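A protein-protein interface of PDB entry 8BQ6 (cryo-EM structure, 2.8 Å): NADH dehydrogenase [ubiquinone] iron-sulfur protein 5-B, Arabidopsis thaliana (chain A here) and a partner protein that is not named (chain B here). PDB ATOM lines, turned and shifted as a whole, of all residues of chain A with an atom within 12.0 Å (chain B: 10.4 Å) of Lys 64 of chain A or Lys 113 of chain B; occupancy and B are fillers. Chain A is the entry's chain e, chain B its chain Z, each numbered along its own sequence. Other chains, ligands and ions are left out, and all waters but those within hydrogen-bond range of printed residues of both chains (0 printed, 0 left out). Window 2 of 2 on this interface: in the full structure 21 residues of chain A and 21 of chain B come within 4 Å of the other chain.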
ATOM      1  N   ARG A  53     -13.782  12.646 -12.458  1.00  0.00           N
ATOM      2  CA  ARG A  53     -12.349  12.657 -12.734  1.00  0.00           C
ATOM      3  C   ARG A  53     -11.943  13.866 -13.579  1.00  0.00           C
ATOM      4  O   ARG A  53     -10.917  14.514 -13.311  1.00  0.00           O
ATOM      5  CB  ARG A  53     -11.961  11.356 -13.427  1.00  0.00           C
ATOM      6  CG  ARG A  53     -10.687  11.437 -14.219  1.00  0.00           C
ATOM      7  CD  ARG A  53     -10.700  10.436 -15.356  1.00  0.00           C
ATOM      8  NE  ARG A  53      -9.359  10.095 -15.812  1.00  0.00           N
ATOM      9  CZ  ARG A  53      -8.438   9.506 -15.060  1.00  0.00           C
ATOM     10  NH1 ARG A  53      -8.674   9.182 -13.798  1.00  0.00           N
ATOM     11  NH2 ARG A  53      -7.254   9.220 -15.591  1.00  0.00           N
ATOM     12  N   ASN A  55     -13.455  16.690 -13.658  1.00  0.00           N
ATOM     13  CA  ASN A  55     -13.547  17.857 -12.794  1.00  0.00           C
ATOM     14  C   ASN A  55     -12.350  17.946 -11.864  1.00  0.00           C
ATOM     15  O   ASN A  55     -11.903  19.050 -11.547  1.00  0.00           O
ATOM     16  CB  ASN A  55     -14.848  17.826 -12.001  1.00  0.00           C
ATOM     17  CG  ASN A  55     -16.060  18.075 -12.873  1.00  0.00           C
ATOM     18  OD1 ASN A  55     -15.937  18.504 -14.019  1.00  0.00           O
ATOM     19  ND2 ASN A  55     -17.240  17.830 -12.325  1.00  0.00           N
ATOM     20  N   ARG A  56     -11.826  16.802 -11.415  1.00  0.00           N
ATOM     21  CA  ARG A  56     -10.573  16.805 -10.663  1.00  0.00           C
ATOM     22  C   ARG A  56      -9.452  17.431 -11.477  1.00  0.00           C
ATOM     23  O   ARG A  56      -8.673  18.245 -10.962  1.00  0.00           O
ATOM     24  CB  ARG A  56     -10.182  15.383 -10.273  1.00  0.00           C
ATOM     25  CG  ARG A  56     -11.139  14.680  -9.353  1.00  0.00           C
ATOM     26  CD  ARG A  56     -10.380  13.794  -8.387  1.00  0.00           C
ATOM     27  NE  ARG A  56     -11.256  13.229  -7.371  1.00  0.00           N
ATOM     28  CZ  ARG A  56     -12.037  12.173  -7.557  1.00  0.00           C
ATOM     29  NH1 ARG A  56     -12.054  11.521  -8.709  1.00  0.00           N
ATOM     30  NH2 ARG A  56     -12.820  11.763  -6.565  1.00  0.00           N
ATOM     31  N   ILE A  57      -9.347  17.046 -12.750  1.00  0.00           N
ATOM     32  CA  ILE A  57      -8.311  17.620 -13.609  1.00  0.00           C
ATOM     33  C   ILE A  57      -8.494  19.129 -13.725  1.00  0.00           C
ATOM     34  O   ILE A  57      -7.538  19.906 -13.603  1.00  0.00           O
ATOM     35  CB  ILE A  57      -8.323  16.949 -14.992  1.00  0.00           C
ATOM     36  CG1 ILE A  57      -7.691  15.562 -14.905  1.00  0.00           C
ATOM     37  CG2 ILE A  57      -7.597  17.813 -16.014  1.00  0.00           C
ATOM     38  CD1 ILE A  57      -8.229  14.601 -15.921  1.00  0.00           C
ATOM     39  N   TYR A  58      -9.733  19.564 -13.955  1.00  0.00           N
ATOM     40  CA  TYR A  58     -10.002  20.991 -14.092  1.00  0.00           C
ATOM     41  C   TYR A  58      -9.683  21.745 -12.802  1.00  0.00           C
ATOM     42  O   TYR A  58      -9.130  22.851 -12.836  1.00  0.00           O
ATOM     43  CB  TYR A  58     -11.458  21.189 -14.503  1.00  0.00           C
ATOM     44  CG  TYR A  58     -12.038  22.523 -14.127  1.00  0.00           C
ATOM     45  CD1 TYR A  58     -11.826  23.643 -14.917  1.00  0.00           C
ATOM     46  CD2 TYR A  58     -12.795  22.666 -12.974  1.00  0.00           C
ATOM     47  CE1 TYR A  58     -12.360  24.865 -14.571  1.00  0.00           C
ATOM     48  CE2 TYR A  58     -13.326  23.879 -12.619  1.00  0.00           C
ATOM     49  CZ  TYR A  58     -13.108  24.975 -13.419  1.00  0.00           C
ATOM     50  OH  TYR A  58     -13.647  26.183 -13.056  1.00  0.00           O
ATOM     51  N   LYS A  59     -10.031  21.158 -11.655  1.00  0.00           N
ATOM     52  CA  LYS A  59      -9.751  21.770 -10.361  1.00  0.00           C
ATOM     53  C   LYS A  59      -8.254  21.919 -10.137  1.00  0.00           C
ATOM     54  O   LYS A  59      -7.788  22.949  -9.640  1.00  0.00           O
ATOM     55  CB  LYS A  59     -10.370  20.919  -9.253  1.00  0.00           C
ATOM     56  CG  LYS A  59     -10.829  21.676  -8.029  1.00  0.00           C
ATOM     57  CD  LYS A  59     -11.999  20.955  -7.388  1.00  0.00           C
ATOM     58  CE  LYS A  59     -12.098  21.250  -5.901  1.00  0.00           C
ATOM     59  NZ  LYS A  59     -12.153  19.993  -5.108  1.00  0.00           N
ATOM     60  N   GLU A  60      -7.484  20.886 -10.483  1.00  0.00           N
ATOM     61  CA  GLU A  60      -6.034  20.970 -10.344  1.00  0.00           C
ATOM     62  C   GLU A  60      -5.452  22.034 -11.262  1.00  0.00           C
ATOM     63  O   GLU A  60      -4.511  22.744 -10.885  1.00  0.00           O
ATOM     64  CB  GLU A  60      -5.397  19.617 -10.630  1.00  0.00           C
ATOM     65  CG  GLU A  60      -5.204  18.776  -9.397  1.00  0.00           C
ATOM     66  CD  GLU A  60      -4.088  19.310  -8.530  1.00  0.00           C
ATOM     67  OE1 GLU A  60      -3.002  19.591  -9.077  1.00  0.00           O
ATOM     68  OE2 GLU A  60      -4.293  19.440  -7.304  1.00  0.00           O
ATOM     69  N   GLU A  61      -5.987  22.143 -12.480  1.00  0.00           N
ATOM     70  CA  GLU A  61      -5.556  23.208 -13.380  1.00  0.00           C
ATOM     71  C   GLU A  61      -5.835  24.581 -12.781  1.00  0.00           C
ATOM     72  O   GLU A  61      -4.983  25.475 -12.836  1.00  0.00           O
ATOM     73  CB  GLU A  61      -6.253  23.068 -14.732  1.00  0.00           C
ATOM     74  CG  GLU A  61      -5.815  24.093 -15.764  1.00  0.00           C
ATOM     75  CD  GLU A  61      -6.494  23.891 -17.106  1.00  0.00           C
ATOM     76  OE1 GLU A  61      -7.333  22.973 -17.217  1.00  0.00           O
ATOM     77  OE2 GLU A  61      -6.190  24.651 -18.051  1.00  0.00           O
ATOM     78  N   GLN A  62      -7.024  24.769 -12.206  1.00  0.00           N
ATOM     79  CA  GLN A  62      -7.346  26.050 -11.583  1.00  0.00           C
ATOM     80  C   GLN A  62      -6.471  26.320 -10.366  1.00  0.00           C
ATOM     81  O   GLN A  62      -6.148  27.478 -10.080  1.00  0.00           O
ATOM     82  CB  GLN A  62      -8.820  26.092 -11.181  1.00  0.00           C
ATOM     83  CG  GLN A  62      -9.586  27.312 -11.679  1.00  0.00           C
ATOM     84  CD  GLN A  62      -9.698  27.358 -13.193  1.00  0.00           C
ATOM     85  OE1 GLN A  62      -9.641  26.328 -13.862  1.00  0.00           O
ATOM     86  NE2 GLN A  62      -9.879  28.555 -13.738  1.00  0.00           N
ATOM     87  N   ARG A  63      -6.099  25.270  -9.632  1.00  0.00           N
ATOM     88  CA  ARG A  63      -5.259  25.433  -8.452  1.00  0.00           C
ATOM     89  C   ARG A  63      -3.836  25.824  -8.829  1.00  0.00           C
ATOM     90  O   ARG A  63      -3.224  26.673  -8.172  1.00  0.00           O
ATOM     91  CB  ARG A  63      -5.253  24.142  -7.641  1.00  0.00           C
ATOM     92  CG  ARG A  63      -4.947  24.335  -6.178  1.00  0.00           C
ATOM     93  CD  ARG A  63      -3.917  23.330  -5.716  1.00  0.00           C
ATOM     94  NE  ARG A  63      -2.671  23.433  -6.468  1.00  0.00           N
ATOM     95  CZ  ARG A  63      -1.655  22.590  -6.343  1.00  0.00           C
ATOM     96  NH1 ARG A  63      -1.719  21.548  -5.534  1.00  0.00           N
ATOM     97  NH2 ARG A  63      -0.546  22.803  -7.046  1.00  0.00           N
ATOM     98  N   LYS A  64      -3.298  25.220  -9.887  1.00  0.00           N
ATOM     99  CA  LYS A  64      -1.964  25.539 -10.382  1.00  0.00           C
ATOM    100  C   LYS A  64      -1.948  26.786 -11.256  1.00  0.00           C
ATOM    101  O   LYS A  64      -1.026  26.962 -12.064  1.00  0.00           O
ATOM    102  CB  LYS A  64      -1.392  24.347 -11.147  1.00  0.00           C
ATOM    103  CG  LYS A  64      -1.022  23.168 -10.269  1.00  0.00           C
ATOM    104  CD  LYS A  64      -0.428  22.052 -11.104  1.00  0.00           C
ATOM    105  CE  LYS A  64       0.661  21.308 -10.359  1.00  0.00           C
ATOM    106  NZ  LYS A  64       1.574  20.621 -11.313  1.00  0.00           N
ATOM    107  N   LEU A  65      -2.949  27.649 -11.134  1.00  0.00           N
ATOM    108  CA  LEU A  65      -3.006  28.848 -11.956  1.00  0.00           C
ATOM    109  C   LEU A  65      -3.274  30.087 -11.109  1.00  0.00           C
ATOM    110  O   LEU A  65      -4.350  30.236 -10.531  1.00  0.00           O
ATOM    111  CB  LEU A  65      -4.080  28.702 -13.034  1.00  0.00           C
ATOM    112  CG  LEU A  65      -4.184  29.861 -14.025  1.00  0.00           C
ATOM    113  CD1 LEU A  65      -2.858  30.064 -14.736  1.00  0.00           C
ATOM    114  CD2 LEU A  65      -5.300  29.616 -15.022  1.00  0.00           C
ATOM    115  N   LEU B 105      -3.754  13.297 -23.654  1.00  0.00           N
ATOM    116  CA  LEU B 105      -3.101  12.500 -22.624  1.00  0.00           C
ATOM    117  C   LEU B 105      -1.811  13.162 -22.159  1.00  0.00           C
ATOM    118  O   LEU B 105      -1.505  13.164 -20.959  1.00  0.00           O
ATOM    119  CB  LEU B 105      -2.839  11.093 -23.155  1.00  0.00           C
ATOM    120  CG  LEU B 105      -3.339   9.950 -22.279  1.00  0.00           C
ATOM    121  CD1 LEU B 105      -4.704  10.295 -21.716  1.00  0.00           C
ATOM    122  CD2 LEU B 105      -3.413   8.675 -23.092  1.00  0.00           C
ATOM    123  N   GLU B 106      -1.048  13.743 -23.089  1.00  0.00           N
ATOM    124  CA  GLU B 106       0.121  14.517 -22.676  1.00  0.00           C
ATOM    125  C   GLU B 106      -0.290  15.714 -21.824  1.00  0.00           C
ATOM    126  O   GLU B 106       0.346  16.006 -20.801  1.00  0.00           O
ATOM    127  CB  GLU B 106       0.944  14.971 -23.887  1.00  0.00           C
ATOM    128  CG  GLU B 106       1.045  13.963 -25.020  1.00  0.00           C
ATOM    129  CD  GLU B 106       1.652  14.549 -26.284  1.00  0.00           C
ATOM    130  OE1 GLU B 106       2.685  14.020 -26.749  1.00  0.00           O
ATOM    131  OE2 GLU B 106       1.106  15.543 -26.809  1.00  0.00           O
ATOM    132  N   TYR B 107      -1.364  16.406 -22.216  1.00  0.00           N
ATOM    133  CA  TYR B 107      -1.857  17.528 -21.416  1.00  0.00           C
ATOM    134  C   TYR B 107      -2.247  17.087 -20.007  1.00  0.00           C
ATOM    135  O   TYR B 107      -1.919  17.754 -19.018  1.00  0.00           O
ATOM    136  CB  TYR B 107      -3.048  18.187 -22.113  1.00  0.00           C
ATOM    137  CG  TYR B 107      -3.936  18.981 -21.178  1.00  0.00           C
ATOM    138  CD1 TYR B 107      -5.203  18.524 -20.842  1.00  0.00           C
ATOM    139  CD2 TYR B 107      -3.504  20.173 -20.621  1.00  0.00           C
ATOM    140  CE1 TYR B 107      -6.016  19.240 -19.986  1.00  0.00           C
ATOM    141  CE2 TYR B 107      -4.313  20.894 -19.771  1.00  0.00           C
ATOM    142  CZ  TYR B 107      -5.565  20.422 -19.453  1.00  0.00           C
ATOM    143  OH  TYR B 107      -6.375  21.134 -18.599  1.00  0.00           O
ATOM    144  N   GLU B 108      -2.967  15.970 -19.900  1.00  0.00           N
ATOM    145  CA  GLU B 108      -3.387  15.474 -18.593  1.00  0.00           C
ATOM    146  C   GLU B 108      -2.190  15.079 -17.739  1.00  0.00           C
ATOM    147  O   GLU B 108      -2.154  15.374 -16.538  1.00  0.00           O
ATOM    148  CB  GLU B 108      -4.339  14.293 -18.771  1.00  0.00           C
ATOM    149  CG  GLU B 108      -4.597  13.489 -17.515  1.00  0.00           C
ATOM    150  CD  GLU B 108      -5.739  12.509 -17.691  1.00  0.00           C
ATOM    151  OE1 GLU B 108      -6.747  12.882 -18.328  1.00  0.00           O
ATOM    152  OE2 GLU B 108      -5.633  11.371 -17.191  1.00  0.00           O
ATOM    153  N   ALA B 109      -1.204  14.408 -18.339  1.00  0.00           N
ATOM    154  CA  ALA B 109      -0.002  14.053 -17.592  1.00  0.00           C
ATOM    155  C   ALA B 109       0.709  15.299 -17.091  1.00  0.00           C
ATOM    156  O   ALA B 109       1.208  15.329 -15.960  1.00  0.00           O
ATOM    157  CB  ALA B 109       0.932  13.215 -18.464  1.00  0.00           C
ATOM    158  N   ASP B 110       0.759  16.340 -17.921  1.00  0.00           N
ATOM    159  CA  ASP B 110       1.397  17.584 -17.512  1.00  0.00           C
ATOM    160  C   ASP B 110       0.667  18.219 -16.334  1.00  0.00           C
ATOM    161  O   ASP B 110       1.272  18.496 -15.291  1.00  0.00           O
ATOM    162  CB  ASP B 110       1.436  18.544 -18.696  1.00  0.00           C
ATOM    163  CG  ASP B 110       2.619  19.468 -18.652  1.00  0.00           C
ATOM    164  OD1 ASP B 110       2.569  20.458 -17.893  1.00  0.00           O
ATOM    165  OD2 ASP B 110       3.592  19.210 -19.388  1.00  0.00           O
ATOM    166  N   VAL B 111      -0.644  18.427 -16.474  1.00  0.00           N
ATOM    167  CA  VAL B 111      -1.400  19.128 -15.440  1.00  0.00           C
ATOM    168  C   VAL B 111      -1.432  18.315 -14.152  1.00  0.00           C
ATOM    169  O   VAL B 111      -1.208  18.848 -13.058  1.00  0.00           O
ATOM    170  CB  VAL B 111      -2.820  19.449 -15.944  1.00  0.00           C
ATOM    171  CG1 VAL B 111      -3.763  19.676 -14.774  1.00  0.00           C
ATOM    172  CG2 VAL B 111      -2.800  20.658 -16.860  1.00  0.00           C
ATOM    173  N   MET B 112      -1.687  17.014 -14.262  1.00  0.00           N
ATOM    174  CA  MET B 112      -1.833  16.144 -13.102  1.00  0.00           C
ATOM    175  C   MET B 112      -0.503  15.661 -12.548  1.00  0.00           C
ATOM    176  O   MET B 112      -0.492  14.823 -11.641  1.00  0.00           O
ATOM    177  CB  MET B 112      -2.709  14.942 -13.450  1.00  0.00           C
ATOM    178  CG  MET B 112      -4.140  15.311 -13.757  1.00  0.00           C
ATOM    179  SD  MET B 112      -4.942  16.121 -12.367  1.00  0.00           S
ATOM    180  CE  MET B 112      -4.994  14.770 -11.198  1.00  0.00           C
ATOM    181  N   LYS B 113       0.610  16.146 -13.082  1.00  0.00           N
ATOM    182  CA  LYS B 113       1.897  15.874 -12.464  1.00  0.00           C
ATOM    183  C   LYS B 113       1.927  16.468 -11.062  1.00  0.00           C
ATOM    184  O   LYS B 113       1.300  17.498 -10.798  1.00  0.00           O
ATOM    185  CB  LYS B 113       3.018  16.458 -13.318  1.00  0.00           C
ATOM    186  CG  LYS B 113       4.379  15.885 -13.025  1.00  0.00           C
ATOM    187  CD  LYS B 113       5.389  16.439 -14.001  1.00  0.00           C
ATOM    188  CE  LYS B 113       5.529  17.941 -13.829  1.00  0.00           C
ATOM    189  NZ  LYS B 113       5.322  18.657 -15.118  1.00  0.00           N
ATOM    190  N   ASP B 114       2.638  15.794 -10.157  1.00  0.00           N
ATOM    191  CA  ASP B 114       2.777  16.184  -8.756  1.00  0.00           C
ATOM    192  C   ASP B 114       1.515  15.927  -7.941  1.00  0.00           C
ATOM    193  O   ASP B 114       1.439  16.330  -6.777  1.00  0.00           O
ATOM    194  CB  ASP B 114       3.193  17.654  -8.611  1.00  0.00           C
ATOM    195  CG  ASP B 114       4.684  17.825  -8.456  1.00  0.00           C
ATOM    196  OD1 ASP B 114       5.309  16.986  -7.777  1.00  0.00           O
ATOM    197  OD2 ASP B 114       5.236  18.789  -9.025  1.00  0.00           O
ATOM    198  N   VAL B 115       0.514  15.273  -8.519  1.00  0.00           N
ATOM    199  CA  VAL B 115      -0.666  14.845  -7.779  1.00  0.00           C
ATOM    200  C   VAL B 115      -0.522  13.347  -7.520  1.00  0.00           C
ATOM    201  O   VAL B 115      -0.534  12.551  -8.470  1.00  0.00           O
ATOM    202  CB  VAL B 115      -1.966  15.162  -8.531  1.00  0.00           C
ATOM    203  CG1 VAL B 115      -3.139  15.148  -7.572  1.00  0.00           C
ATOM    204  CG2 VAL B 115      -1.867  16.513  -9.212  1.00  0.00           C
ATOM    205  N   PRO B 116      -0.364  12.921  -6.271  1.00  0.00           N
ATOM    206  CA  PRO B 116      -0.091  11.505  -6.003  1.00  0.00           C
ATOM    207  C   PRO B 116      -1.320  10.636  -6.216  1.00  0.00           C
ATOM    208  O   PRO B 116      -2.450  11.024  -5.911  1.00  0.00           O
ATOM    209  CB  PRO B 116       0.335  11.505  -4.533  1.00  0.00           C
ATOM    210  CG  PRO B 116      -0.395  12.675  -3.950  1.00  0.00           C
ATOM    211  CD  PRO B 116      -0.438  13.718  -5.034  1.00  0.00           C
ATOM    212  N   GLY B 117      -1.077   9.433  -6.737  1.00  0.00           N
ATOM    213  CA  GLY B 117      -2.129   8.469  -6.979  1.00  0.00           C
ATOM    214  C   GLY B 117      -2.823   8.594  -8.315  1.00  0.00           C
ATOM    215  O   GLY B 117      -3.622   7.715  -8.665  1.00  0.00           O
ATOM    216  N   TRP B 118      -2.547   9.644  -9.078  1.00  0.00           N
ATOM    217  CA  TRP B 118      -3.176   9.773 -10.378  1.00  0.00           C
ATOM    218  C   TRP B 118      -2.648   8.711 -11.340  1.00  0.00           C
ATOM    219  O   TRP B 118      -1.493   8.285 -11.269  1.00  0.00           O
ATOM    220  CB  TRP B 118      -2.941  11.166 -10.954  1.00  0.00           C
ATOM    221  CG  TRP B 118      -4.000  11.566 -11.910  1.00  0.00           C
ATOM    222  CD1 TRP B 118      -3.864  11.742 -13.253  1.00  0.00           C
ATOM    223  CD2 TRP B 118      -5.373  11.825 -11.605  1.00  0.00           C
ATOM    224  NE1 TRP B 118      -5.066  12.103 -13.806  1.00  0.00           N
ATOM    225  CE2 TRP B 118      -6.010  12.162 -12.814  1.00  0.00           C
ATOM    226  CE3 TRP B 118      -6.126  11.811 -10.428  1.00  0.00           C
ATOM    227  CZ2 TRP B 118      -7.363  12.482 -12.882  1.00  0.00           C
ATOM    228  CZ3 TRP B 118      -7.470  12.128 -10.496  1.00  0.00           C
ATOM    229  CH2 TRP B 118      -8.075  12.460 -11.714  1.00  0.00           C
ATOM    230  N   LYS B 119      -3.533   8.260 -12.225  1.00  0.00           N
ATOM    231  CA  LYS B 119      -3.162   7.394 -13.338  1.00  0.00           C
ATOM    232  C   LYS B 119      -3.683   8.041 -14.607  1.00  0.00           C
ATOM    233  O   LYS B 119      -4.892   8.243 -14.748  1.00  0.00           O
ATOM    234  CB  LYS B 119      -3.733   5.982 -13.180  1.00  0.00           C
ATOM    235  CG  LYS B 119      -2.744   4.955 -12.648  1.00  0.00           C
ATOM    236  CD  LYS B 119      -1.370   5.123 -13.284  1.00  0.00           C
ATOM    237  CE  LYS B 119      -1.239   4.315 -14.568  1.00  0.00           C
ATOM    238  NZ  LYS B 119       0.177   4.206 -15.013  1.00  0.00           N
ATOM    239  N   VAL B 120      -2.775   8.361 -15.528  1.00  0.00           N
ATOM    240  CA  VAL B 120      -3.149   9.122 -16.712  1.00  0.00           C
ATOM    241  C   VAL B 120      -3.955   8.243 -17.656  1.00  0.00           C
ATOM    242  O   VAL B 120      -3.552   7.118 -17.982  1.00  0.00           O
ATOM    243  CB  VAL B 120      -1.899   9.689 -17.401  1.00  0.00           C
ATOM    244  CG1 VAL B 120      -2.251  10.247 -18.770  1.00  0.00           C
ATOM    245  CG2 VAL B 120      -1.271  10.765 -16.536  1.00  0.00           C
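The backbone carbonyl oxygen of Lys 113 of chain B lies within hydrogen-bond range of the side-chain amino group of Lys 64 of chain A. The guanidinium group (NH2) of Arg 53 of chain A is in hydrogen-bond range of the backbone carbonyl oxygen (O) of Lys 119 of chain B, at 2.7 Å. OE2 of Glu 108 of chain B is in salt-bridge range of NH2 of Arg 53 of chain A (3.1 Å). OE1 of Glu 61 of chain A lies within hydrogen-bond range of OH of Tyr 107 of chain B, 2.5 Å away.
The side-chain carboxylate (OE2) of Glu 60 of chain A is in salt-bridge range of the guanidinium group (NH1) of Arg 63 of chain A, 3.8 Å away.
Among the printed residues, merely in contact across the chains: Arg 53 of chain A with Trp 118 of chain B, Arg 56 of chain A with Trp 118 of chain B, Ile 57 of chain A with Glu 108 of chain B, Ile 57 of chain A with Val 111 of chain B, Ile 57 of chain A with Met 112 of chain B, Ile 57 of chain A with Trp 118 of chain B, Glu 60 of chain A with Met 112 of chain B, Glu 60 of chain A with Val 115 of chain B and Lys 64 of chain A with Val 111 of chain B.
Of chain B, only Val 111 (3.7 Å) and Lys 113 (3.2 Å) come within 4 Å of Lys 64 of chain A. Of chain A, only Lys 64 comes within 4 Å of Lys 113 of chain B. No residue of chain B comes within 4 Å of Arg 63 of chain A. No residue of chain A comes within 4 Å of Asp 110 of chain B. Of chain A, only Ile 57 (3.96 Å) and Lys 64 (3.7 Å) come within 4 Å of Val 111 of chain B. Of chain A, only Glu 60 (3.3 Å) comes within 4 Å of Val 115 of chain B. Printed residues of chain B within 4 Å of Arg 53 of chain A: Glu 108, Trp 118 and Lys 119. Of the printed residues of chain A, Lys 119 of chain B touches Arg 53 (2.7 Å). The nearest residue of chain B that does not touch Lys 64 of chain A is Asp 114 of chain B (4.3 Å). The nearest printed residue of chain A that does not touch Glu 108 of chain B is Glu 60 of chain A (8.0 Å).
Of the 16 printed residues of chain B, 8 touch a printed residue of chain A. Printed residues of chain B that touch a printed residue of chain A: Tyr 107, Glu 108, Val 111, Met 112, Lys 113, Val 115, Trp 118 and Lys 119. Hydrophobic or aromatic side chains of chain B within 4 Å of the printed part of chain A: Tyr 107, Val 111, Met 112, Val 115 and Trp 118. Of the 12 printed residues of chain A, 6 touch a printed residue of chain B. Hydrophobic or aromatic side chains of chain A that line the printed part of chain B: Ile 57. Among the printed residues, Asp or Glu carboxylates within 4 Å of a Lys or Arg side-chain nitrogen of the other chain: Arg 53 of chain A with Glu 108 of chain B (3.1 Å).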
